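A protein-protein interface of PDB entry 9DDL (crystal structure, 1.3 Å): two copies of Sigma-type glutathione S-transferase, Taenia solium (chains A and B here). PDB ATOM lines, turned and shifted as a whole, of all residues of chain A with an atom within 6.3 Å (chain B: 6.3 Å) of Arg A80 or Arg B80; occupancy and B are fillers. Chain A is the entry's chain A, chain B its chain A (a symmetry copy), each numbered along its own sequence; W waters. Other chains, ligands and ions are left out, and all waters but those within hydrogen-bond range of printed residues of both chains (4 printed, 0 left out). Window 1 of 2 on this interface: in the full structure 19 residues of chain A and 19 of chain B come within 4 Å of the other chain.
OE1 of Glu A100 is in salt-bridge range of NH1 of Arg B80 (3.2 Å).
The side-chain carboxylate (OE1) of Glu B100 is in salt-bridge range of the guanidinium group (NH1) of Arg A80.
The side-chain carboxylate (OE2) of Glu A100 is in salt-bridge range of the guanidinium group (NH2) of Arg B84 (2.9 Å).
The guanidinium group (NH2) of Arg A84 lies within salt-bridge range of the side-chain carboxylate (OE2) of Glu B100.
NH2 of Arg B80 lies close to NH2 of Arg A80.
The side-chain hydroxyl (OH) of Tyr A89 sits at hydrogen-bond distance from the side-chain carboxylate (OE2) of Glu A100, 2.6 Å away.
The side-chain carboxylate (OE2) of Glu B100 is in hydrogen-bond range of the side-chain hydroxyl (OH) of Tyr B89 (2.6 Å).
Among the printed residues, pairs that only touch across the chains: Arg A84 with Arg B84 (3.5 Å), Ala A77 with Arg B101 (3.8 Å), Arg A101 with Ala B77 (3.8 Å), Glu A100 with Ala B77 (3.9 Å) and Ala A77 with Glu B100 (3.9 Å).
Of chain B, only Arg B80 (3.3 Å) and Glu B100 (3.2 Å) come within 4 Å of Arg A80.
Of the printed residues of chain A, Arg B84 touches Arg A84 (3.5 Å) and Glu A100 (2.9 Å).
Of the printed residues of chain A, Arg B101 touches Ala A77 (3.8 Å).
The nearest residue of chain B that does not touch Arg A80 is Tyr B89 (5.7 Å).
The nearest printed residue of chain B that does not touch Ala A77 is Asn B103 (7.4 Å).
Of the 17 printed residues of chain B, 5 touch a printed residue of chain A.
Of the 17 printed residues of chain A, 5 touch a printed residue of chain B.
Along chain A the printed residues that touch a printed residue of chain B span positions 77 to 101.
Among the printed residues, 10 pairs touch across the chains.
Among the printed residues, Asp or Glu carboxylates within 4 Å of a Lys or Arg side-chain nitrogen of the other chain: Arg A80 with Glu B100 (3.2 Å), Arg A84 with Glu B100 (2.9 Å), Glu A100 with Arg B80 (3.2 Å) and Glu A100 with Arg B84 (2.9 Å).
Ala A77 touches Glu B100, and with the chains exchanged Glu A100 touches Ala B77.
Ala A77 touches Arg B101, and with the chains exchanged Arg A101 touches Ala B77.
Arg A80 touches its own counterpart, Arg B80.
Arg A84 touches Glu B100, and with the chains exchanged Glu A100 touches Arg B84.
Of the 10 pairs that touch across the chains among the printed residues, 10 have their exchanged pair printed and touching as well.
Water W3 lies within hydrogen-bond range of the side-chain carboxylate (OE1) of Glu A100 (2.7 Å), the backbone carbonyl oxygen (O) of Ala B77 (2.8 Å) and the guanidinium group (NH1) of Arg B84 (3.4 Å).
Water W1 lies within hydrogen-bond range of OE1 of Glu B100 (2.7 Å), O of Ala A77 (2.8 Å) and NH1 of Arg A84 (3.4 Å).
Water W4 bridges NH1 of Arg B80 (2.8 Å) and O of Glu A100 (2.9 Å).
Water W2 bridges NH1 of Arg A80 (2.8 Å) and O of Glu B100 (2.9 Å).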
ATOM      1  N   VAL A  27     -21.688 -23.159 -43.610  1.00  0.00           N
ATOM      2  CA  VAL A  27     -22.681 -23.571 -42.610  1.00  0.00           C
ATOM      3  C   VAL A  27     -24.073 -23.143 -43.044  1.00  0.00           C
ATOM      4  O   VAL A  27     -25.029 -23.930 -42.976  1.00  0.00           O
ATOM      5  CB  VAL A  27     -22.358 -22.975 -41.225  1.00  0.00           C
ATOM      6  CG1 VAL A  27     -23.550 -23.214 -40.249  1.00  0.00           C
ATOM      7  CG2 VAL A  27     -21.100 -23.565 -40.683  1.00  0.00           C
ATOM      8  N   SER A  75     -14.886 -14.845 -36.177  1.00  0.00           N
ATOM      9  CA  SER A  75     -15.341 -15.740 -37.238  1.00  0.00           C
ATOM     10  C   SER A  75     -15.675 -17.143 -36.740  1.00  0.00           C
ATOM     11  O   SER A  75     -16.721 -17.704 -37.096  1.00  0.00           O
ATOM     12  CB  SER A  75     -14.303 -15.796 -38.364  1.00  0.00           C
ATOM     13  OG  SER A  75     -13.037 -16.202 -37.871  1.00  0.00           O
ATOM     14  N   MET A  76     -14.785 -17.753 -35.949  1.00  0.00           N
ATOM     15  CA  MET A  76     -15.054 -19.120 -35.514  1.00  0.00           C
ATOM     16  C   MET A  76     -16.156 -19.192 -34.466  1.00  0.00           C
ATOM     17  O   MET A  76     -16.920 -20.168 -34.452  1.00  0.00           O
ATOM     18  CB  MET A  76     -13.768 -19.790 -35.013  1.00  0.00           C
ATOM     19  CG  MET A  76     -13.759 -21.310 -35.097  1.00  0.00           C
ATOM     20  SD  MET A  76     -14.124 -21.967 -36.739  1.00  0.00           S
ATOM     21  CE  MET A  76     -13.711 -23.687 -36.502  1.00  0.00           C
ATOM     22  N   ALA A  77     -16.274 -18.184 -33.595  1.00  0.00           N
ATOM     23  CA  ALA A  77     -17.397 -18.149 -32.663  1.00  0.00           C
ATOM     24  C   ALA A  77     -18.723 -18.066 -33.412  1.00  0.00           C
ATOM     25  O   ALA A  77     -19.696 -18.745 -33.047  1.00  0.00           O
ATOM     26  CB  ALA A  77     -17.258 -16.957 -31.704  1.00  0.00           C
ATOM     27  N   ILE A  78     -18.772 -17.259 -34.474  1.00  0.00           N
ATOM     28  CA  ILE A  78     -19.962 -17.163 -35.310  1.00  0.00           C
ATOM     29  C   ILE A  78     -20.252 -18.505 -35.966  1.00  0.00           C
ATOM     30  O   ILE A  78     -21.384 -18.989 -35.933  1.00  0.00           O
ATOM     31  CB  ILE A  78     -19.771 -16.066 -36.366  1.00  0.00           C
ATOM     32  CG1 ILE A  78     -19.632 -14.703 -35.707  1.00  0.00           C
ATOM     33  CG2 ILE A  78     -20.951 -16.088 -37.345  1.00  0.00           C
ATOM     34  CD1 ILE A  78     -19.098 -13.663 -36.685  1.00  0.00           C
ATOM     35  N   ALA A  79     -19.236 -19.132 -36.555  1.00  0.00           N
ATOM     36  CA  ALA A  79     -19.446 -20.404 -37.236  1.00  0.00           C
ATOM     37  C   ALA A  79     -19.975 -21.475 -36.286  1.00  0.00           C
ATOM     38  O   ALA A  79     -20.857 -22.247 -36.664  1.00  0.00           O
ATOM     39  CB  ALA A  79     -18.152 -20.868 -37.913  1.00  0.00           C
ATOM     40  N   ARG A  80     -19.410 -21.577 -35.076  1.00  0.00           N
ATOM     41  CA  ARG A  80     -19.858 -22.591 -34.128  1.00  0.00           C
ATOM     42  C   ARG A  80     -21.274 -22.308 -33.646  1.00  0.00           C
ATOM     43  O   ARG A  80     -22.084 -23.228 -33.505  1.00  0.00           O
ATOM     44  CB  ARG A  80     -18.887 -22.669 -32.944  1.00  0.00           C
ATOM     45  CG  ARG A  80     -17.496 -23.152 -33.281  1.00  0.00           C
ATOM     46  CD  ARG A  80     -16.758 -23.483 -31.991  1.00  0.00           C
ATOM     47  NE  ARG A  80     -15.312 -23.318 -32.109  1.00  0.00           N
ATOM     48  CZ  ARG A  80     -14.653 -22.223 -31.752  1.00  0.00           C
ATOM     49  NH1 ARG A  80     -15.286 -21.148 -31.298  1.00  0.00           N
ATOM     50  NH2 ARG A  80     -13.327 -22.190 -31.885  1.00  0.00           N
ATOM     51  N   LEU A  81     -21.601 -21.043 -33.395  1.00  0.00           N
ATOM     52  CA  LEU A  81     -22.962 -20.693 -33.000  1.00  0.00           C
ATOM     53  C   LEU A  81     -23.959 -21.105 -34.076  1.00  0.00           C
ATOM     54  O   LEU A  81     -25.020 -21.671 -33.780  1.00  0.00           O
ATOM     55  CB  LEU A  81     -23.013 -19.187 -32.762  1.00  0.00           C
ATOM     56  CG  LEU A  81     -24.407 -18.612 -32.564  1.00  0.00           C
ATOM     57  CD1 LEU A  81     -25.128 -19.217 -31.346  1.00  0.00           C
ATOM     58  CD2 LEU A  81     -24.309 -17.096 -32.427  1.00  0.00           C
ATOM     59  N   LEU A  82     -23.644 -20.804 -35.340  1.00  0.00           N
ATOM     60  CA  LEU A  82     -24.542 -21.183 -36.425  1.00  0.00           C
ATOM     61  C   LEU A  82     -24.594 -22.693 -36.568  1.00  0.00           C
ATOM     62  O   LEU A  82     -25.670 -23.258 -36.783  1.00  0.00           O
ATOM     63  CB  LEU A  82     -24.087 -20.526 -37.722  1.00  0.00           C
ATOM     64  CG  LEU A  82     -24.221 -19.006 -37.716  1.00  0.00           C
ATOM     65  CD1 LEU A  82     -23.517 -18.493 -38.966  1.00  0.00           C
ATOM     66  CD2 LEU A  82     -25.683 -18.568 -37.703  1.00  0.00           C
ATOM     67  N   ALA A  83     -23.458 -23.377 -36.411  1.00  0.00           N
ATOM     68  CA  ALA A  83     -23.484 -24.832 -36.516  1.00  0.00           C
ATOM     69  C   ALA A  83     -24.361 -25.443 -35.428  1.00  0.00           C
ATOM     70  O   ALA A  83     -25.144 -26.369 -35.691  1.00  0.00           O
ATOM     71  CB  ALA A  83     -22.072 -25.407 -36.458  1.00  0.00           C
ATOM     72  N   ARG A  84     -24.251 -24.940 -34.192  1.00  0.00           N
ATOM     73  CA  ARG A  84     -25.095 -25.457 -33.122  1.00  0.00           C
ATOM     74  C   ARG A  84     -26.563 -25.217 -33.428  1.00  0.00           C
ATOM     75  O   ARG A  84     -27.406 -26.090 -33.185  1.00  0.00           O
ATOM     76  CB  ARG A  84     -24.745 -24.776 -31.806  1.00  0.00           C
ATOM     77  CG  ARG A  84     -23.393 -25.184 -31.260  1.00  0.00           C
ATOM     78  CD  ARG A  84     -23.062 -24.419 -29.977  1.00  0.00           C
ATOM     79  NE  ARG A  84     -21.765 -24.857 -29.466  1.00  0.00           N
ATOM     80  CZ  ARG A  84     -20.628 -24.169 -29.568  1.00  0.00           C
ATOM     81  NH1 ARG A  84     -20.610 -22.915 -30.026  1.00  0.00           N
ATOM     82  NH2 ARG A  84     -19.480 -24.742 -29.180  1.00  0.00           N
ATOM     83  N   THR A  85     -26.880 -24.051 -33.967  1.00  0.00           N
ATOM     84  CA  THR A  85     -28.272 -23.702 -34.233  1.00  0.00           C
ATOM     85  C   THR A  85     -28.884 -24.652 -35.244  1.00  0.00           C
ATOM     86  O   THR A  85     -30.056 -25.041 -35.124  1.00  0.00           O
ATOM     87  CB  THR A  85     -28.321 -22.295 -34.814  1.00  0.00           C
ATOM     88  OG1 THR A  85     -27.794 -21.363 -33.856  1.00  0.00           O
ATOM     89  CG2 THR A  85     -29.742 -21.896 -35.142  1.00  0.00           C
ATOM     90  N   TYR A  89     -23.229 -29.504 -35.204  1.00  0.00           N
ATOM     91  CA  TYR A  89     -22.188 -29.470 -34.183  1.00  0.00           C
ATOM     92  C   TYR A  89     -22.251 -30.665 -33.243  1.00  0.00           C
ATOM     93  O   TYR A  89     -21.873 -30.557 -32.070  1.00  0.00           O
ATOM     94  CB  TYR A  89     -22.189 -28.145 -33.414  1.00  0.00           C
ATOM     95  CG  TYR A  89     -20.793 -27.741 -32.988  1.00  0.00           C
ATOM     96  CD1 TYR A  89     -19.847 -27.305 -33.926  1.00  0.00           C
ATOM     97  CD2 TYR A  89     -20.412 -27.793 -31.654  1.00  0.00           C
ATOM     98  CE1 TYR A  89     -18.550 -26.960 -33.561  1.00  0.00           C
ATOM     99  CE2 TYR A  89     -19.097 -27.431 -31.282  1.00  0.00           C
ATOM    100  CZ  TYR A  89     -18.180 -27.022 -32.246  1.00  0.00           C
ATOM    101  OH  TYR A  89     -16.898 -26.683 -31.886  1.00  0.00           O
ATOM    102  N   GLU A 100     -13.626 -30.507 -32.604  1.00  0.00           N
ATOM    103  CA  GLU A 100     -12.737 -29.426 -32.205  1.00  0.00           C
ATOM    104  C   GLU A 100     -11.279 -29.830 -32.305  1.00  0.00           C
ATOM    105  O   GLU A 100     -10.430 -28.978 -32.579  1.00  0.00           O
ATOM    106  CB  GLU A 100     -13.093 -28.952 -30.795  1.00  0.00           C
ATOM    107  CG  GLU A 100     -14.425 -28.213 -30.813  1.00  0.00           C
ATOM    108  CD  GLU A 100     -14.933 -27.766 -29.470  1.00  0.00           C
ATOM    109  OE1 GLU A 100     -14.324 -28.081 -28.418  1.00  0.00           O
ATOM    110  OE2 GLU A 100     -15.980 -27.070 -29.487  1.00  0.00           O
ATOM    111  N   ARG A 101     -10.961 -31.107 -32.108  1.00  0.00           N
ATOM    112  CA  ARG A 101      -9.598 -31.552 -32.375  1.00  0.00           C
ATOM    113  C   ARG A 101      -9.259 -31.346 -33.841  1.00  0.00           C
ATOM    114  O   ARG A 101      -8.219 -30.762 -34.182  1.00  0.00           O
ATOM    115  CB  ARG A 101      -9.447 -33.022 -31.997  1.00  0.00           C
ATOM    116  CG  ARG A 101      -8.009 -33.536 -32.158  1.00  0.00           C
ATOM    117  CD  ARG A 101      -7.929 -35.003 -31.771  1.00  0.00           C
ATOM    118  NE  ARG A 101      -8.646 -35.840 -32.726  1.00  0.00           N
ATOM    119  CZ  ARG A 101      -8.793 -37.152 -32.612  1.00  0.00           C
ATOM    120  NH1 ARG A 101      -8.293 -37.817 -31.581  1.00  0.00           N
ATOM    121  NH2 ARG A 101      -9.460 -37.812 -33.554  1.00  0.00           N
ATOM    122  N   ASN A 103     -10.784 -29.351 -36.024  1.00  0.00           N
ATOM    123  CA  ASN A 103     -10.767 -27.936 -36.380  1.00  0.00           C
ATOM    124  C   ASN A 103      -9.531 -27.233 -35.856  1.00  0.00           C
ATOM    125  O   ASN A 103      -9.050 -26.293 -36.495  1.00  0.00           O
ATOM    126  CB  ASN A 103     -12.041 -27.240 -35.907  1.00  0.00           C
ATOM    127  CG  ASN A 103     -13.197 -27.484 -36.848  1.00  0.00           C
ATOM    128  OD1 ASN A 103     -13.006 -27.929 -37.983  1.00  0.00           O
ATOM    129  ND2 ASN A 103     -14.402 -27.193 -36.389  1.00  0.00           N
ATOM    130  N   LEU A 159     -19.446 -29.172 -38.530  1.00  0.00           N
ATOM    131  CA  LEU A 159     -18.547 -28.061 -38.851  1.00  0.00           C
ATOM    132  C   LEU A 159     -17.150 -28.508 -39.272  1.00  0.00           C
ATOM    133  O   LEU A 159     -16.532 -27.861 -40.127  1.00  0.00           O
ATOM    134  CB  LEU A 159     -18.466 -27.100 -37.657  1.00  0.00           C
ATOM    135  CG  LEU A 159     -17.780 -25.774 -37.976  1.00  0.00           C
ATOM    136  CD1 LEU A 159     -18.634 -24.940 -38.910  1.00  0.00           C
ATOM    137  CD2 LEU A 159     -17.452 -25.018 -36.671  1.00  0.00           C
ATOM    138  N   VAL B  27      -8.939 -25.368 -15.335  1.00  0.00           N
ATOM    139  CA  VAL B  27     -10.234 -26.058 -15.390  1.00  0.00           C
ATOM    140  C   VAL B  27     -10.278 -27.176 -14.362  1.00  0.00           C
ATOM    141  O   VAL B  27     -11.266 -27.323 -13.626  1.00  0.00           O
ATOM    142  CB  VAL B  27     -10.504 -26.627 -16.796  1.00  0.00           C
ATOM    143  CG1 VAL B  27     -11.752 -27.562 -16.764  1.00  0.00           C
ATOM    144  CG2 VAL B  27     -10.692 -25.523 -17.781  1.00  0.00           C
ATOM    145  N   SER B  75      -4.718 -28.381 -27.324  1.00  0.00           N
ATOM    146  CA  SER B  75      -4.900 -27.793 -26.000  1.00  0.00           C
ATOM    147  C   SER B  75      -6.299 -27.223 -25.782  1.00  0.00           C
ATOM    148  O   SER B  75      -6.920 -27.464 -24.737  1.00  0.00           O
ATOM    149  CB  SER B  75      -3.832 -26.724 -25.745  1.00  0.00           C
ATOM    150  OG  SER B  75      -3.861 -25.723 -26.749  1.00  0.00           O
ATOM    151  N   MET B  76      -6.803 -26.429 -26.732  1.00  0.00           N
ATOM    152  CA  MET B  76      -8.113 -25.819 -26.515  1.00  0.00           C
ATOM    153  C   MET B  76      -9.250 -26.824 -26.637  1.00  0.00           C
ATOM    154  O   MET B  76     -10.253 -26.699 -25.921  1.00  0.00           O
ATOM    155  CB  MET B  76      -8.319 -24.630 -27.462  1.00  0.00           C
ATOM    156  CG  MET B  76      -9.308 -23.582 -26.973  1.00  0.00           C
ATOM    157  SD  MET B  76      -8.947 -22.927 -25.330  1.00  0.00           S
ATOM    158  CE  MET B  76     -10.091 -21.558 -25.265  1.00  0.00           C
ATOM    159  N   ALA B  77      -9.122 -27.828 -27.512  1.00  0.00           N
ATOM    160  CA  ALA B  77     -10.126 -28.886 -27.565  1.00  0.00           C
ATOM    161  C   ALA B  77     -10.193 -29.639 -26.240  1.00  0.00           C
ATOM    162  O   ALA B  77     -11.289 -29.955 -25.750  1.00  0.00           O
ATOM    163  CB  ALA B  77      -9.815 -29.861 -28.710  1.00  0.00           C
ATOM    164  N   ILE B  78      -9.034 -29.912 -25.637  1.00  0.00           N
ATOM    165  CA  ILE B  78      -8.983 -30.555 -24.331  1.00  0.00           C
ATOM    166  C   ILE B  78      -9.640 -29.670 -23.284  1.00  0.00           C
ATOM    167  O   ILE B  78     -10.475 -30.131 -22.503  1.00  0.00           O
ATOM    168  CB  ILE B  78      -7.527 -30.860 -23.956  1.00  0.00           C
ATOM    169  CG1 ILE B  78      -6.921 -31.865 -24.922  1.00  0.00           C
ATOM    170  CG2 ILE B  78      -7.468 -31.378 -22.513  1.00  0.00           C
ATOM    171  CD1 ILE B  78      -5.403 -31.918 -24.793  1.00  0.00           C
ATOM    172  N   ALA B  79      -9.290 -28.385 -23.259  1.00  0.00           N
ATOM    173  CA  ALA B  79      -9.851 -27.484 -22.259  1.00  0.00           C
ATOM    174  C   ALA B  79     -11.371 -27.398 -22.362  1.00  0.00           C
ATOM    175  O   ALA B  79     -12.054 -27.379 -21.337  1.00  0.00           O
ATOM    176  CB  ALA B  79      -9.218 -26.093 -22.378  1.00  0.00           C
ATOM    177  N   ARG B  80     -11.914 -27.286 -23.581  1.00  0.00           N
ATOM    178  CA  ARG B  80     -13.360 -27.182 -23.747  1.00  0.00           C
ATOM    179  C   ARG B  80     -14.053 -28.480 -23.356  1.00  0.00           C
ATOM    180  O   ARG B  80     -15.113 -28.459 -22.725  1.00  0.00           O
ATOM    181  CB  ARG B  80     -13.697 -26.800 -25.192  1.00  0.00           C
ATOM    182  CG  ARG B  80     -13.236 -25.426 -25.621  1.00  0.00           C
ATOM    183  CD  ARG B  80     -13.909 -25.064 -26.938  1.00  0.00           C
ATOM    184  NE  ARG B  80     -13.110 -24.149 -27.748  1.00  0.00           N
ATOM    185  CZ  ARG B  80     -12.288 -24.532 -28.717  1.00  0.00           C
ATOM    186  NH1 ARG B  80     -12.088 -25.815 -28.992  1.00  0.00           N
ATOM    187  NH2 ARG B  80     -11.622 -23.607 -29.408  1.00  0.00           N
ATOM    188  N   LEU B  81     -13.473 -29.623 -23.712  1.00  0.00           N
ATOM    189  CA  LEU B  81     -14.046 -30.903 -23.308  1.00  0.00           C
ATOM    190  C   LEU B  81     -14.119 -31.006 -21.790  1.00  0.00           C
ATOM    191  O   LEU B  81     -15.135 -31.438 -21.227  1.00  0.00           O
ATOM    192  CB  LEU B  81     -13.175 -32.015 -23.885  1.00  0.00           C
ATOM    193  CG  LEU B  81     -13.491 -33.412 -23.376  1.00  0.00           C
ATOM    194  CD1 LEU B  81     -14.932 -33.847 -23.701  1.00  0.00           C
ATOM    195  CD2 LEU B  81     -12.491 -34.400 -23.967  1.00  0.00           C
ATOM    196  N   LEU B  82     -13.033 -30.633 -21.105  1.00  0.00           N
ATOM    197  CA  LEU B  82     -13.037 -30.688 -19.647  1.00  0.00           C
ATOM    198  C   LEU B  82     -14.010 -29.671 -19.080  1.00  0.00           C
ATOM    199  O   LEU B  82     -14.730 -29.970 -18.124  1.00  0.00           O
ATOM    200  CB  LEU B  82     -11.627 -30.448 -19.121  1.00  0.00           C
ATOM    201  CG  LEU B  82     -10.645 -31.560 -19.477  1.00  0.00           C
ATOM    202  CD1 LEU B  82      -9.256 -31.067 -19.093  1.00  0.00           C
ATOM    203  CD2 LEU B  82     -10.975 -32.860 -18.749  1.00  0.00           C
ATOM    204  N   ALA B  83     -14.087 -28.478 -19.675  1.00  0.00           N
ATOM    205  CA  ALA B  83     -15.034 -27.491 -19.168  1.00  0.00           C
ATOM    206  C   ALA B  83     -16.469 -27.992 -19.300  1.00  0.00           C
ATOM    207  O   ALA B  83     -17.284 -27.834 -18.377  1.00  0.00           O
ATOM    208  CB  ALA B  83     -14.862 -26.154 -19.881  1.00  0.00           C
ATOM    209  N   ARG B  84     -16.806 -28.604 -20.442  1.00  0.00           N
ATOM    210  CA  ARG B  84     -18.151 -29.140 -20.607  1.00  0.00           C
ATOM    211  C   ARG B  84     -18.432 -30.221 -19.579  1.00  0.00           C
ATOM    212  O   ARG B  84     -19.534 -30.283 -19.018  1.00  0.00           O
ATOM    213  CB  ARG B  84     -18.311 -29.729 -22.002  1.00  0.00           C
ATOM    214  CG  ARG B  84     -18.336 -28.682 -23.096  1.00  0.00           C
ATOM    215  CD  ARG B  84     -18.427 -29.333 -24.479  1.00  0.00           C
ATOM    216  NE  ARG B  84     -18.476 -28.294 -25.505  1.00  0.00           N
ATOM    217  CZ  ARG B  84     -17.459 -27.946 -26.294  1.00  0.00           C
ATOM    218  NH1 ARG B  84     -16.321 -28.644 -26.314  1.00  0.00           N
ATOM    219  NH2 ARG B  84     -17.591 -26.885 -27.102  1.00  0.00           N
ATOM    220  N   THR B  85     -17.450 -31.067 -19.314  1.00  0.00           N
ATOM    221  CA  THR B  85     -17.647 -32.180 -18.391  1.00  0.00           C
ATOM    222  C   THR B  85     -17.964 -31.677 -16.997  1.00  0.00           C
ATOM    223  O   THR B  85     -18.801 -32.254 -16.287  1.00  0.00           O
ATOM    224  CB  THR B  85     -16.360 -32.992 -18.323  1.00  0.00           C
ATOM    225  OG1 THR B  85     -16.061 -33.526 -19.622  1.00  0.00           O
ATOM    226  CG2 THR B  85     -16.500 -34.141 -17.349  1.00  0.00           C
ATOM    227  N   TYR B  89     -18.905 -24.557 -18.985  1.00  0.00           N
ATOM    228  CA  TYR B  89     -19.039 -24.156 -20.381  1.00  0.00           C
ATOM    229  C   TYR B  89     -20.440 -23.664 -20.716  1.00  0.00           C
ATOM    230  O   TYR B  89     -20.896 -23.811 -21.857  1.00  0.00           O
ATOM    231  CB  TYR B  89     -18.584 -25.262 -21.338  1.00  0.00           C
ATOM    232  CG  TYR B  89     -17.963 -24.696 -22.598  1.00  0.00           C
ATOM    233  CD1 TYR B  89     -16.707 -24.073 -22.570  1.00  0.00           C
ATOM    234  CD2 TYR B  89     -18.623 -24.778 -23.816  1.00  0.00           C
ATOM    235  CE1 TYR B  89     -16.132 -23.518 -23.708  1.00  0.00           C
ATOM    236  CE2 TYR B  89     -18.032 -24.224 -24.975  1.00  0.00           C
ATOM    237  CZ  TYR B  89     -16.793 -23.596 -24.903  1.00  0.00           C
ATOM    238  OH  TYR B  89     -16.225 -23.045 -26.027  1.00  0.00           O
ATOM    239  N   GLU B 100     -17.031 -18.035 -26.329  1.00  0.00           N
ATOM    240  CA  GLU B 100     -16.145 -18.262 -27.461  1.00  0.00           C
ATOM    241  C   GLU B 100     -15.741 -16.964 -28.130  1.00  0.00           C
ATOM    242  O   GLU B 100     -14.634 -16.874 -28.666  1.00  0.00           O
ATOM    243  CB  GLU B 100     -16.803 -19.224 -28.452  1.00  0.00           C
ATOM    244  CG  GLU B 100     -16.854 -20.628 -27.863  1.00  0.00           C
ATOM    245  CD  GLU B 100     -17.555 -21.657 -28.706  1.00  0.00           C
ATOM    246  OE1 GLU B 100     -18.132 -21.326 -29.771  1.00  0.00           O
ATOM    247  OE2 GLU B 100     -17.514 -22.836 -28.273  1.00  0.00           O
ATOM    248  N   ARG B 101     -16.599 -15.945 -28.105  1.00  0.00           N
ATOM    249  CA  ARG B 101     -16.165 -14.636 -28.581  1.00  0.00           C
ATOM    250  C   ARG B 101     -15.014 -14.126 -27.730  1.00  0.00           C
ATOM    251  O   ARG B 101     -13.970 -13.707 -28.251  1.00  0.00           O
ATOM    252  CB  ARG B 101     -17.332 -13.655 -28.539  1.00  0.00           C
ATOM    253  CG  ARG B 101     -16.976 -12.279 -29.119  1.00  0.00           C
ATOM    254  CD  ARG B 101     -18.177 -11.350 -29.043  1.00  0.00           C
ATOM    255  NE  ARG B 101     -18.493 -11.010 -27.661  1.00  0.00           N
ATOM    256  CZ  ARG B 101     -19.524 -10.264 -27.289  1.00  0.00           C
ATOM    257  NH1 ARG B 101     -20.375  -9.768 -28.175  1.00  0.00           N
ATOM    258  NH2 ARG B 101     -19.705 -10.013 -25.996  1.00  0.00           N
ATOM    259  N   ASN B 103     -13.009 -15.890 -25.746  1.00  0.00           N
ATOM    260  CA  ASN B 103     -11.822 -16.726 -25.888  1.00  0.00           C
ATOM    261  C   ASN B 103     -11.121 -16.497 -27.212  1.00  0.00           C
ATOM    262  O   ASN B 103      -9.894 -16.616 -27.279  1.00  0.00           O
ATOM    263  CB  ASN B 103     -12.166 -18.200 -25.692  1.00  0.00           C
ATOM    264  CG  ASN B 103     -12.272 -18.563 -24.230  1.00  0.00           C
ATOM    265  OD1 ASN B 103     -11.826 -17.812 -23.358  1.00  0.00           O
ATOM    266  ND2 ASN B 103     -12.857 -19.715 -23.949  1.00  0.00           N
ATOM    267  N   LEU B 159     -15.103 -21.241 -18.795  1.00  0.00           N
ATOM    268  CA  LEU B 159     -13.767 -21.278 -19.397  1.00  0.00           C
ATOM    269  C   LEU B 159     -13.230 -19.901 -19.775  1.00  0.00           C
ATOM    270  O   LEU B 159     -12.019 -19.668 -19.676  1.00  0.00           O
ATOM    271  CB  LEU B 159     -13.779 -22.205 -20.620  1.00  0.00           C
ATOM    272  CG  LEU B 159     -12.387 -22.533 -21.159  1.00  0.00           C
ATOM    273  CD1 LEU B 159     -11.629 -23.413 -20.185  1.00  0.00           C
ATOM    274  CD2 LEU B 159     -12.499 -23.184 -22.553  1.00  0.00           C
HETATM  275  O   HOH W   1     -20.098 -19.591 -30.401  1.00  0.00           O
HETATM  276  O   HOH W   2     -13.699 -19.153 -30.156  1.00  0.00           O
HETATM  277  O   HOH W   3     -13.601 -30.414 -27.275  1.00  0.00           O
HETATM  278  O   HOH W   4     -10.716 -26.387 -31.357  1.00  0.00           O
